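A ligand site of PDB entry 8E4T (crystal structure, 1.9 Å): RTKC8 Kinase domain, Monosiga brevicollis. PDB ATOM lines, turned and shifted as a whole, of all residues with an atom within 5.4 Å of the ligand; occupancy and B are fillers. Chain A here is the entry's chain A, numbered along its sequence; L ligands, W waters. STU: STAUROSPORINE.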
ATOM      1  N   LEU A  21      -8.140  -2.379 -20.811  1.00  0.00           N
ATOM      2  CA  LEU A  21      -8.970  -3.168 -21.728  1.00  0.00           C
ATOM      3  C   LEU A  21     -10.442  -3.194 -21.340  1.00  0.00           C
ATOM      4  O   LEU A  21     -11.313  -3.165 -22.202  1.00  0.00           O
ATOM      5  CB  LEU A  21      -8.457  -4.612 -21.808  1.00  0.00           C
ATOM      6  CG  LEU A  21      -7.146  -4.874 -22.561  1.00  0.00           C
ATOM      7  CD1 LEU A  21      -6.762  -6.341 -22.431  1.00  0.00           C
ATOM      8  CD2 LEU A  21      -7.270  -4.448 -24.029  1.00  0.00           C
ATOM      9  N   GLY A  22     -10.734  -3.268 -20.047  1.00  0.00           N
ATOM     10  CA  GLY A  22     -12.111  -3.311 -19.592  1.00  0.00           C
ATOM     11  C   GLY A  22     -12.180  -3.133 -18.098  1.00  0.00           C
ATOM     12  O   GLY A  22     -11.353  -3.672 -17.354  1.00  0.00           O
ATOM     13  N   GLN A  23     -13.150  -2.348 -17.637  1.00  0.00           N
ATOM     14  CA  GLN A  23     -13.362  -2.098 -16.221  1.00  0.00           C
ATOM     15  C   GLN A  23     -14.782  -2.498 -15.850  1.00  0.00           C
ATOM     16  O   GLN A  23     -15.719  -2.325 -16.635  1.00  0.00           O
ATOM     17  CB  GLN A  23     -13.124  -0.632 -15.850  1.00  0.00           C
ATOM     18  CG  GLN A  23     -13.212  -0.389 -14.361  1.00  0.00           C
ATOM     19  CD  GLN A  23     -13.019   1.051 -13.957  1.00  0.00           C
ATOM     20  OE1 GLN A  23     -13.513   1.473 -12.916  1.00  0.00           O
ATOM     21  NE2 GLN A  23     -12.300   1.812 -14.783  1.00  0.00           N
ATOM     22  N   PHE A  26     -16.170  -6.108 -11.060  1.00  0.00           N
ATOM     23  CA  PHE A  26     -15.222  -7.173 -10.759  1.00  0.00           C
ATOM     24  C   PHE A  26     -13.835  -6.618 -10.460  1.00  0.00           C
ATOM     25  O   PHE A  26     -13.129  -7.122  -9.578  1.00  0.00           O
ATOM     26  CB  PHE A  26     -15.157  -8.163 -11.933  1.00  0.00           C
ATOM     27  CG  PHE A  26     -14.446  -7.598 -13.147  1.00  0.00           C
ATOM     28  CD1 PHE A  26     -15.108  -6.791 -14.042  1.00  0.00           C
ATOM     29  CD2 PHE A  26     -13.106  -7.877 -13.370  1.00  0.00           C
ATOM     30  CE1 PHE A  26     -14.453  -6.268 -15.141  1.00  0.00           C
ATOM     31  CE2 PHE A  26     -12.450  -7.356 -14.453  1.00  0.00           C
ATOM     32  CZ  PHE A  26     -13.123  -6.557 -15.348  1.00  0.00           C
ATOM     33  N   VAL A  29      -9.137  -4.937 -16.099  1.00  0.00           N
ATOM     34  CA  VAL A  29      -8.260  -5.739 -16.951  1.00  0.00           C
ATOM     35  C   VAL A  29      -7.449  -4.777 -17.794  1.00  0.00           C
ATOM     36  O   VAL A  29      -8.014  -3.905 -18.478  1.00  0.00           O
ATOM     37  CB  VAL A  29      -9.047  -6.723 -17.841  1.00  0.00           C
ATOM     38  CG1 VAL A  29      -8.087  -7.460 -18.798  1.00  0.00           C
ATOM     39  CG2 VAL A  29      -9.830  -7.723 -17.007  1.00  0.00           C
ATOM     40  N   ALA A  45      -2.705  -9.848 -21.061  1.00  0.00           N
ATOM     41  CA  ALA A  45      -3.722  -9.122 -20.313  1.00  0.00           C
ATOM     42  C   ALA A  45      -3.478  -9.364 -18.833  1.00  0.00           C
ATOM     43  O   ALA A  45      -3.232 -10.506 -18.430  1.00  0.00           O
ATOM     44  CB  ALA A  45      -5.134  -9.560 -20.708  1.00  0.00           C
ATOM     45  N   LYS A  47      -5.197  -8.858 -15.060  1.00  0.00           N
ATOM     46  CA  LYS A  47      -6.429  -8.606 -14.325  1.00  0.00           C
ATOM     47  C   LYS A  47      -6.074  -8.297 -12.876  1.00  0.00           C
ATOM     48  O   LYS A  47      -5.283  -9.016 -12.267  1.00  0.00           O
ATOM     49  CB  LYS A  47      -7.347  -9.831 -14.415  1.00  0.00           C
ATOM     50  CG  LYS A  47      -8.708  -9.738 -13.713  1.00  0.00           C
ATOM     51  CD  LYS A  47      -9.546 -10.978 -14.070  1.00  0.00           C
ATOM     52  CE  LYS A  47     -11.061 -10.796 -13.853  1.00  0.00           C
ATOM     53  NZ  LYS A  47     -11.518 -11.005 -12.433  1.00  0.00           N
ATOM     54  N   GLU A  64     -10.103 -17.664  -8.802  1.00  0.00           N
ATOM     55  CA  GLU A  64     -10.277 -17.594 -10.248  1.00  0.00           C
ATOM     56  C   GLU A  64      -9.053 -18.138 -10.970  1.00  0.00           C
ATOM     57  O   GLU A  64      -9.166 -18.952 -11.902  1.00  0.00           O
ATOM     58  CB  GLU A  64     -10.576 -16.160 -10.660  1.00  0.00           C
ATOM     59  CG  GLU A  64     -10.840 -15.924 -12.152  1.00  0.00           C
ATOM     60  CD  GLU A  64     -11.371 -14.518 -12.425  1.00  0.00           C
ATOM     61  OE1 GLU A  64     -11.473 -13.725 -11.460  1.00  0.00           O
ATOM     62  OE2 GLU A  64     -11.688 -14.203 -13.594  1.00  0.00           O
ATOM     63  N   VAL A  77      -9.377 -19.111 -22.807  1.00  0.00           N
ATOM     64  CA  VAL A  77      -8.305 -18.122 -22.609  1.00  0.00           C
ATOM     65  C   VAL A  77      -7.296 -18.669 -21.602  1.00  0.00           C
ATOM     66  O   VAL A  77      -7.657 -19.058 -20.479  1.00  0.00           O
ATOM     67  CB  VAL A  77      -8.892 -16.779 -22.144  1.00  0.00           C
ATOM     68  CG1 VAL A  77      -7.776 -15.841 -21.641  1.00  0.00           C
ATOM     69  CG2 VAL A  77      -9.648 -16.074 -23.274  1.00  0.00           C
ATOM     70  N   LEU A  93      -2.995 -13.257 -18.197  1.00  0.00           N
ATOM     71  CA  LEU A  93      -3.731 -14.141 -19.090  1.00  0.00           C
ATOM     72  C   LEU A  93      -3.309 -13.917 -20.534  1.00  0.00           C
ATOM     73  O   LEU A  93      -2.704 -12.896 -20.878  1.00  0.00           O
ATOM     74  CB  LEU A  93      -5.251 -13.917 -18.983  1.00  0.00           C
ATOM     75  CG  LEU A  93      -5.899 -13.906 -17.606  1.00  0.00           C
ATOM     76  CD1 LEU A  93      -7.342 -13.410 -17.678  1.00  0.00           C
ATOM     77  CD2 LEU A  93      -5.848 -15.293 -16.999  1.00  0.00           C
ATOM     78  N   GLU A  94      -3.679 -14.865 -21.392  1.00  0.00           N
ATOM     79  CA  GLU A  94      -3.468 -14.737 -22.822  1.00  0.00           C
ATOM     80  C   GLU A  94      -4.171 -13.494 -23.366  1.00  0.00           C
ATOM     81  O   GLU A  94      -5.291 -13.173 -22.979  1.00  0.00           O
ATOM     82  CB  GLU A  94      -3.967 -16.017 -23.519  1.00  0.00           C
ATOM     83  CG  GLU A  94      -3.977 -16.048 -25.034  1.00  0.00           C
ATOM     84  CD  GLU A  94      -4.654 -17.327 -25.561  1.00  0.00           C
ATOM     85  OE1 GLU A  94      -5.234 -18.085 -24.755  1.00  0.00           O
ATOM     86  OE2 GLU A  94      -4.615 -17.573 -26.783  1.00  0.00           O
ATOM     87  N   HIS A  95      -3.485 -12.801 -24.273  1.00  0.00           N
ATOM     88  CA  HIS A  95      -4.022 -11.597 -24.898  1.00  0.00           C
ATOM     89  C   HIS A  95      -4.802 -11.964 -26.149  1.00  0.00           C
ATOM     90  O   HIS A  95      -4.339 -12.763 -26.968  1.00  0.00           O
ATOM     91  CB  HIS A  95      -2.884 -10.638 -25.240  1.00  0.00           C
ATOM     92  CG  HIS A  95      -3.348  -9.355 -25.862  1.00  0.00           C
ATOM     93  ND1 HIS A  95      -3.178  -9.083 -27.199  1.00  0.00           N
ATOM     94  CD2 HIS A  95      -4.012  -8.298 -25.337  1.00  0.00           C
ATOM     95  CE1 HIS A  95      -3.698  -7.898 -27.477  1.00  0.00           C
ATOM     96  NE2 HIS A  95      -4.201  -7.398 -26.357  1.00  0.00           N
ATOM     97  N   MET A  96      -5.992 -11.364 -26.295  1.00  0.00           N
ATOM     98  CA  MET A  96      -6.947 -11.710 -27.366  1.00  0.00           C
ATOM     99  C   MET A  96      -7.154 -10.460 -28.216  1.00  0.00           C
ATOM    100  O   MET A  96      -7.997  -9.620 -27.906  1.00  0.00           O
ATOM    101  CB  MET A  96      -8.292 -12.211 -26.764  1.00  0.00           C
ATOM    102  CG  MET A  96      -8.135 -13.356 -25.763  1.00  0.00           C
ATOM    103  SD  MET A  96      -7.600 -14.861 -26.595  1.00  0.00           S
ATOM    104  CE  MET A  96      -9.029 -15.207 -27.613  1.00  0.00           C
ATOM    105  N   ARG A  97      -6.381 -10.369 -29.301  1.00  0.00           N
ATOM    106  CA  ARG A  97      -6.239  -9.106 -30.030  1.00  0.00           C
ATOM    107  C   ARG A  97      -7.573  -8.585 -30.568  1.00  0.00           C
ATOM    108  O   ARG A  97      -7.757  -7.363 -30.667  1.00  0.00           O
ATOM    109  CB  ARG A  97      -5.236  -9.305 -31.175  1.00  0.00           C
ATOM    110  CG  ARG A  97      -5.196  -8.155 -32.171  1.00  0.00           C
ATOM    111  CD  ARG A  97      -4.480  -8.549 -33.433  1.00  0.00           C
ATOM    112  NE  ARG A  97      -5.053  -7.925 -34.618  1.00  0.00           N
ATOM    113  CZ  ARG A  97      -4.357  -7.628 -35.720  1.00  0.00           C
ATOM    114  NH1 ARG A  97      -3.043  -7.789 -35.774  1.00  0.00           N
ATOM    115  NH2 ARG A  97      -5.003  -7.143 -36.779  1.00  0.00           N
ATOM    116  N   ASN A  98      -8.517  -9.459 -30.929  1.00  0.00           N
ATOM    117  CA  ASN A  98      -9.703  -9.029 -31.670  1.00  0.00           C
ATOM    118  C   ASN A  98     -10.933  -8.818 -30.796  1.00  0.00           C
ATOM    119  O   ASN A  98     -12.033  -8.599 -31.328  1.00  0.00           O
ATOM    120  CB  ASN A  98      -9.981 -10.018 -32.805  1.00  0.00           C
ATOM    121  CG  ASN A  98      -9.177  -9.687 -34.072  1.00  0.00           C
ATOM    122  OD1 ASN A  98      -9.174  -8.548 -34.521  1.00  0.00           O
ATOM    123  ND2 ASN A  98      -8.493 -10.673 -34.616  1.00  0.00           N
ATOM    124  N   GLY A  99     -10.792  -8.855 -29.466  1.00  0.00           N
ATOM    125  CA  GLY A  99     -11.875  -8.422 -28.614  1.00  0.00           C
ATOM    126  C   GLY A  99     -12.992  -9.438 -28.496  1.00  0.00           C
ATOM    127  O   GLY A  99     -12.819 -10.635 -28.768  1.00  0.00           O
ATOM    128  N   SER A 100     -14.163  -8.950 -28.105  1.00  0.00           N
ATOM    129  CA  SER A 100     -15.264  -9.838 -27.777  1.00  0.00           C
ATOM    130  C   SER A 100     -15.986 -10.309 -29.020  1.00  0.00           C
ATOM    131  O   SER A 100     -16.160  -9.555 -29.985  1.00  0.00           O
ATOM    132  CB  SER A 100     -16.261  -9.143 -26.848  1.00  0.00           C
ATOM    133  OG  SER A 100     -17.102  -8.305 -27.615  1.00  0.00           O
ATOM    134  N   ARG A 142     -20.634 -11.583 -25.045  1.00  0.00           N
ATOM    135  CA  ARG A 142     -19.685 -10.609 -24.513  1.00  0.00           C
ATOM    136  C   ARG A 142     -18.592 -11.236 -23.655  1.00  0.00           C
ATOM    137  O   ARG A 142     -17.604 -10.564 -23.350  1.00  0.00           O
ATOM    138  CB  ARG A 142     -20.436  -9.517 -23.723  1.00  0.00           C
ATOM    139  CG  ARG A 142     -21.108  -8.464 -24.620  1.00  0.00           C
ATOM    140  CD  ARG A 142     -21.895  -7.367 -23.874  1.00  0.00           C
ATOM    141  NE  ARG A 142     -21.038  -6.372 -23.239  1.00  0.00           N
ATOM    142  CZ  ARG A 142     -21.498  -5.295 -22.594  1.00  0.00           C
ATOM    143  NH1 ARG A 142     -22.780  -5.037 -22.502  1.00  0.00           N
ATOM    144  NH2 ARG A 142     -20.623  -4.464 -22.037  1.00  0.00           N
ATOM    145  N   ASN A 143     -18.732 -12.506 -23.274  1.00  0.00           N
ATOM    146  CA  ASN A 143     -17.766 -13.187 -22.429  1.00  0.00           C
ATOM    147  C   ASN A 143     -16.883 -14.162 -23.194  1.00  0.00           C
ATOM    148  O   ASN A 143     -16.110 -14.892 -22.581  1.00  0.00           O
ATOM    149  CB  ASN A 143     -18.481 -13.943 -21.314  1.00  0.00           C
ATOM    150  CG  ASN A 143     -18.990 -13.020 -20.217  1.00  0.00           C
ATOM    151  OD1 ASN A 143     -18.439 -11.952 -19.985  1.00  0.00           O
ATOM    152  ND2 ASN A 143     -20.047 -13.444 -19.521  1.00  0.00           N
ATOM    153  N   VAL A 144     -17.003 -14.203 -24.522  1.00  0.00           N
ATOM    154  CA  VAL A 144     -16.135 -14.976 -25.409  1.00  0.00           C
ATOM    155  C   VAL A 144     -15.248 -13.995 -26.166  1.00  0.00           C
ATOM    156  O   VAL A 144     -15.758 -13.006 -26.708  1.00  0.00           O
ATOM    157  CB  VAL A 144     -16.956 -15.832 -26.386  1.00  0.00           C
ATOM    158  CG1 VAL A 144     -16.041 -16.471 -27.470  1.00  0.00           C
ATOM    159  CG2 VAL A 144     -17.780 -16.899 -25.643  1.00  0.00           C
ATOM    160  N   LEU A 145     -13.949 -14.278 -26.228  1.00  0.00           N
ATOM    161  CA  LEU A 145     -12.988 -13.418 -26.911  1.00  0.00           C
ATOM    162  C   LEU A 145     -12.434 -14.099 -28.156  1.00  0.00           C
ATOM    163  O   LEU A 145     -12.473 -15.331 -28.280  1.00  0.00           O
ATOM    164  CB  LEU A 145     -11.849 -13.039 -25.958  1.00  0.00           C
ATOM    165  CG  LEU A 145     -12.349 -12.352 -24.675  1.00  0.00           C
ATOM    166  CD1 LEU A 145     -11.241 -12.204 -23.620  1.00  0.00           C
ATOM    167  CD2 LEU A 145     -13.001 -10.991 -25.001  1.00  0.00           C
ATOM    168  N   ALA A 155     -13.833 -16.913 -21.818  1.00  0.00           N
ATOM    169  CA  ALA A 155     -13.150 -16.097 -20.816  1.00  0.00           C
ATOM    170  C   ALA A 155     -14.093 -15.840 -19.641  1.00  0.00           C
ATOM    171  O   ALA A 155     -15.244 -16.279 -19.617  1.00  0.00           O
ATOM    172  CB  ALA A 155     -12.682 -14.764 -21.436  1.00  0.00           C
ATOM    173  N   ASP A 156     -13.556 -15.125 -18.642  1.00  0.00           N
ATOM    174  CA  ASP A 156     -14.287 -14.653 -17.459  1.00  0.00           C
ATOM    175  C   ASP A 156     -14.829 -15.773 -16.585  1.00  0.00           C
ATOM    176  O   ASP A 156     -16.012 -16.112 -16.653  1.00  0.00           O
ATOM    177  CB  ASP A 156     -15.434 -13.726 -17.861  1.00  0.00           C
ATOM    178  CG  ASP A 156     -15.837 -12.783 -16.737  1.00  0.00           C
ATOM    179  OD1 ASP A 156     -15.540 -13.108 -15.563  1.00  0.00           O
ATOM    180  OD2 ASP A 156     -16.430 -11.725 -17.033  1.00  0.00           O
HETATM  181  O4  STU L   1     -12.856  -6.711 -20.958  1.00  0.00           O
HETATM  182  C25 STU L   1     -12.893  -6.703 -22.347  1.00  0.00           C
HETATM  183  C24 STU L   1     -14.248  -7.132 -22.914  1.00  0.00           C
HETATM  184  C23 STU L   1     -15.251  -7.393 -21.780  1.00  0.00           C
HETATM  185  C22 STU L   1     -14.623  -8.437 -20.838  1.00  0.00           C
HETATM  186  C21 STU L   1     -13.331  -7.845 -20.285  1.00  0.00           C
HETATM  187  C26 STU L   1     -13.717  -7.199 -18.952  1.00  0.00           C
HETATM  188  N2  STU L   1     -12.278  -8.864 -20.099  1.00  0.00           N
HETATM  189  C18 STU L   1     -11.259  -9.056 -21.039  1.00  0.00           C
HETATM  190  C19 STU L   1     -11.007  -8.388 -22.246  1.00  0.00           C
HETATM  191  C6  STU L   1      -9.894  -8.760 -23.024  1.00  0.00           C
HETATM  192  C7  STU L   1      -9.025  -9.801 -22.584  1.00  0.00           C
HETATM  193  C10 STU L   1      -9.299 -10.463 -21.386  1.00  0.00           C
HETATM  194  C11 STU L   1     -10.403 -10.089 -20.614  1.00  0.00           C
HETATM  195  C12 STU L   1     -10.962 -10.556 -19.340  1.00  0.00           C
HETATM  196  C17 STU L   1     -12.104  -9.782 -19.070  1.00  0.00           C
HETATM  197  C16 STU L   1     -12.838 -10.032 -17.887  1.00  0.00           C
HETATM  198  C15 STU L   1     -12.408 -11.036 -17.036  1.00  0.00           C
HETATM  199  C14 STU L   1     -11.270 -11.779 -17.318  1.00  0.00           C
HETATM  200  C13 STU L   1     -10.530 -11.562 -18.472  1.00  0.00           C
HETATM  201  C9  STU L   1      -8.227 -11.509 -21.201  1.00  0.00           C
HETATM  202  N1  STU L   1      -7.346 -11.391 -22.370  1.00  0.00           N
HETATM  203  C8  STU L   1      -7.808 -10.422 -23.172  1.00  0.00           C
HETATM  204  O5  STU L   1      -7.261 -10.092 -24.223  1.00  0.00           O
HETATM  205  C5  STU L   1      -9.944  -7.881 -24.203  1.00  0.00           C
HETATM  206  C20 STU L   1     -11.078  -7.034 -24.050  1.00  0.00           C
HETATM  207  C1  STU L   1     -11.374  -6.074 -25.023  1.00  0.00           C
HETATM  208  C2  STU L   1     -10.532  -5.992 -26.137  1.00  0.00           C
HETATM  209  C3  STU L   1      -9.427  -6.823 -26.274  1.00  0.00           C
HETATM  210  C4  STU L   1      -9.112  -7.773 -25.306  1.00  0.00           C
HETATM  211  N3  STU L   1     -11.711  -7.389 -22.869  1.00  0.00           N
HETATM  212  O6  STU L   1     -14.284  -9.510 -21.686  1.00  0.00           O
HETATM  213  C27 STU L   1     -14.725 -10.742 -21.132  1.00  0.00           C
HETATM  214  N4  STU L   1     -16.551  -7.865 -22.323  1.00  0.00           N
HETATM  215  C28 STU L   1     -17.487  -8.097 -21.194  1.00  0.00           C
HETATM  216  O   HOH W   1     -16.755  -9.466 -18.130  1.00  0.00           O
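An oxygen (O5) of the ligand lies within hydrogen-bond range of the backbone NH of Met 96. The backbone carbonyl oxygen (O) of Arg 142 is in hydrogen-bond range of a nitrogen (N4) of the ligand, 3.1 Å away. O of Glu 94 lies within hydrogen-bond range of N1 of the ligand, at 2.8 Å.
O of Val 29 sits at hydrogen-bond distance from N of Leu 21. The backbone carbonyl oxygen of Gly 22 sits at hydrogen-bond distance from the backbone NH of Val 29 (2.8 Å). The side-chain amino group of Lys 47 lies within salt-bridge range of the side-chain carboxylate of Glu 64 (2.9 Å). O of Ala 45 lies within hydrogen-bond range of N of Leu 93 (2.8 Å).
Leu 21 touches the ligand (O to C25, 3.9 Å). Gly 22 touches the ligand (CA to O4, 3.7 Å). CZ of Phe 26 touches C26 of the ligand, at 3.7 Å. Val 29 touches the ligand (CG2 to C17, 3.7 Å). Ala 45 touches the ligand (CB to N1, 3.3 Å). CE of Lys 47 touches C15 of the ligand, 3.5 Å away. CD1 of Leu 93 touches C13 of the ligand (3.8 Å). His 95 touches the ligand. Gly 99 touches the ligand. Leu 145 touches the ligand (CD1 to C7, 3.4 Å). Asp 156 touches the ligand (CG to C15, 3.9 Å). Hydrophobic or aromatic side chains that line the ligand: Leu 21, Phe 26, Val 29, Ala 45, Leu 93, His 95, Met 96 and Leu 145. Of the 23 residues printed, 14 come within 4 Å of the ligand.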
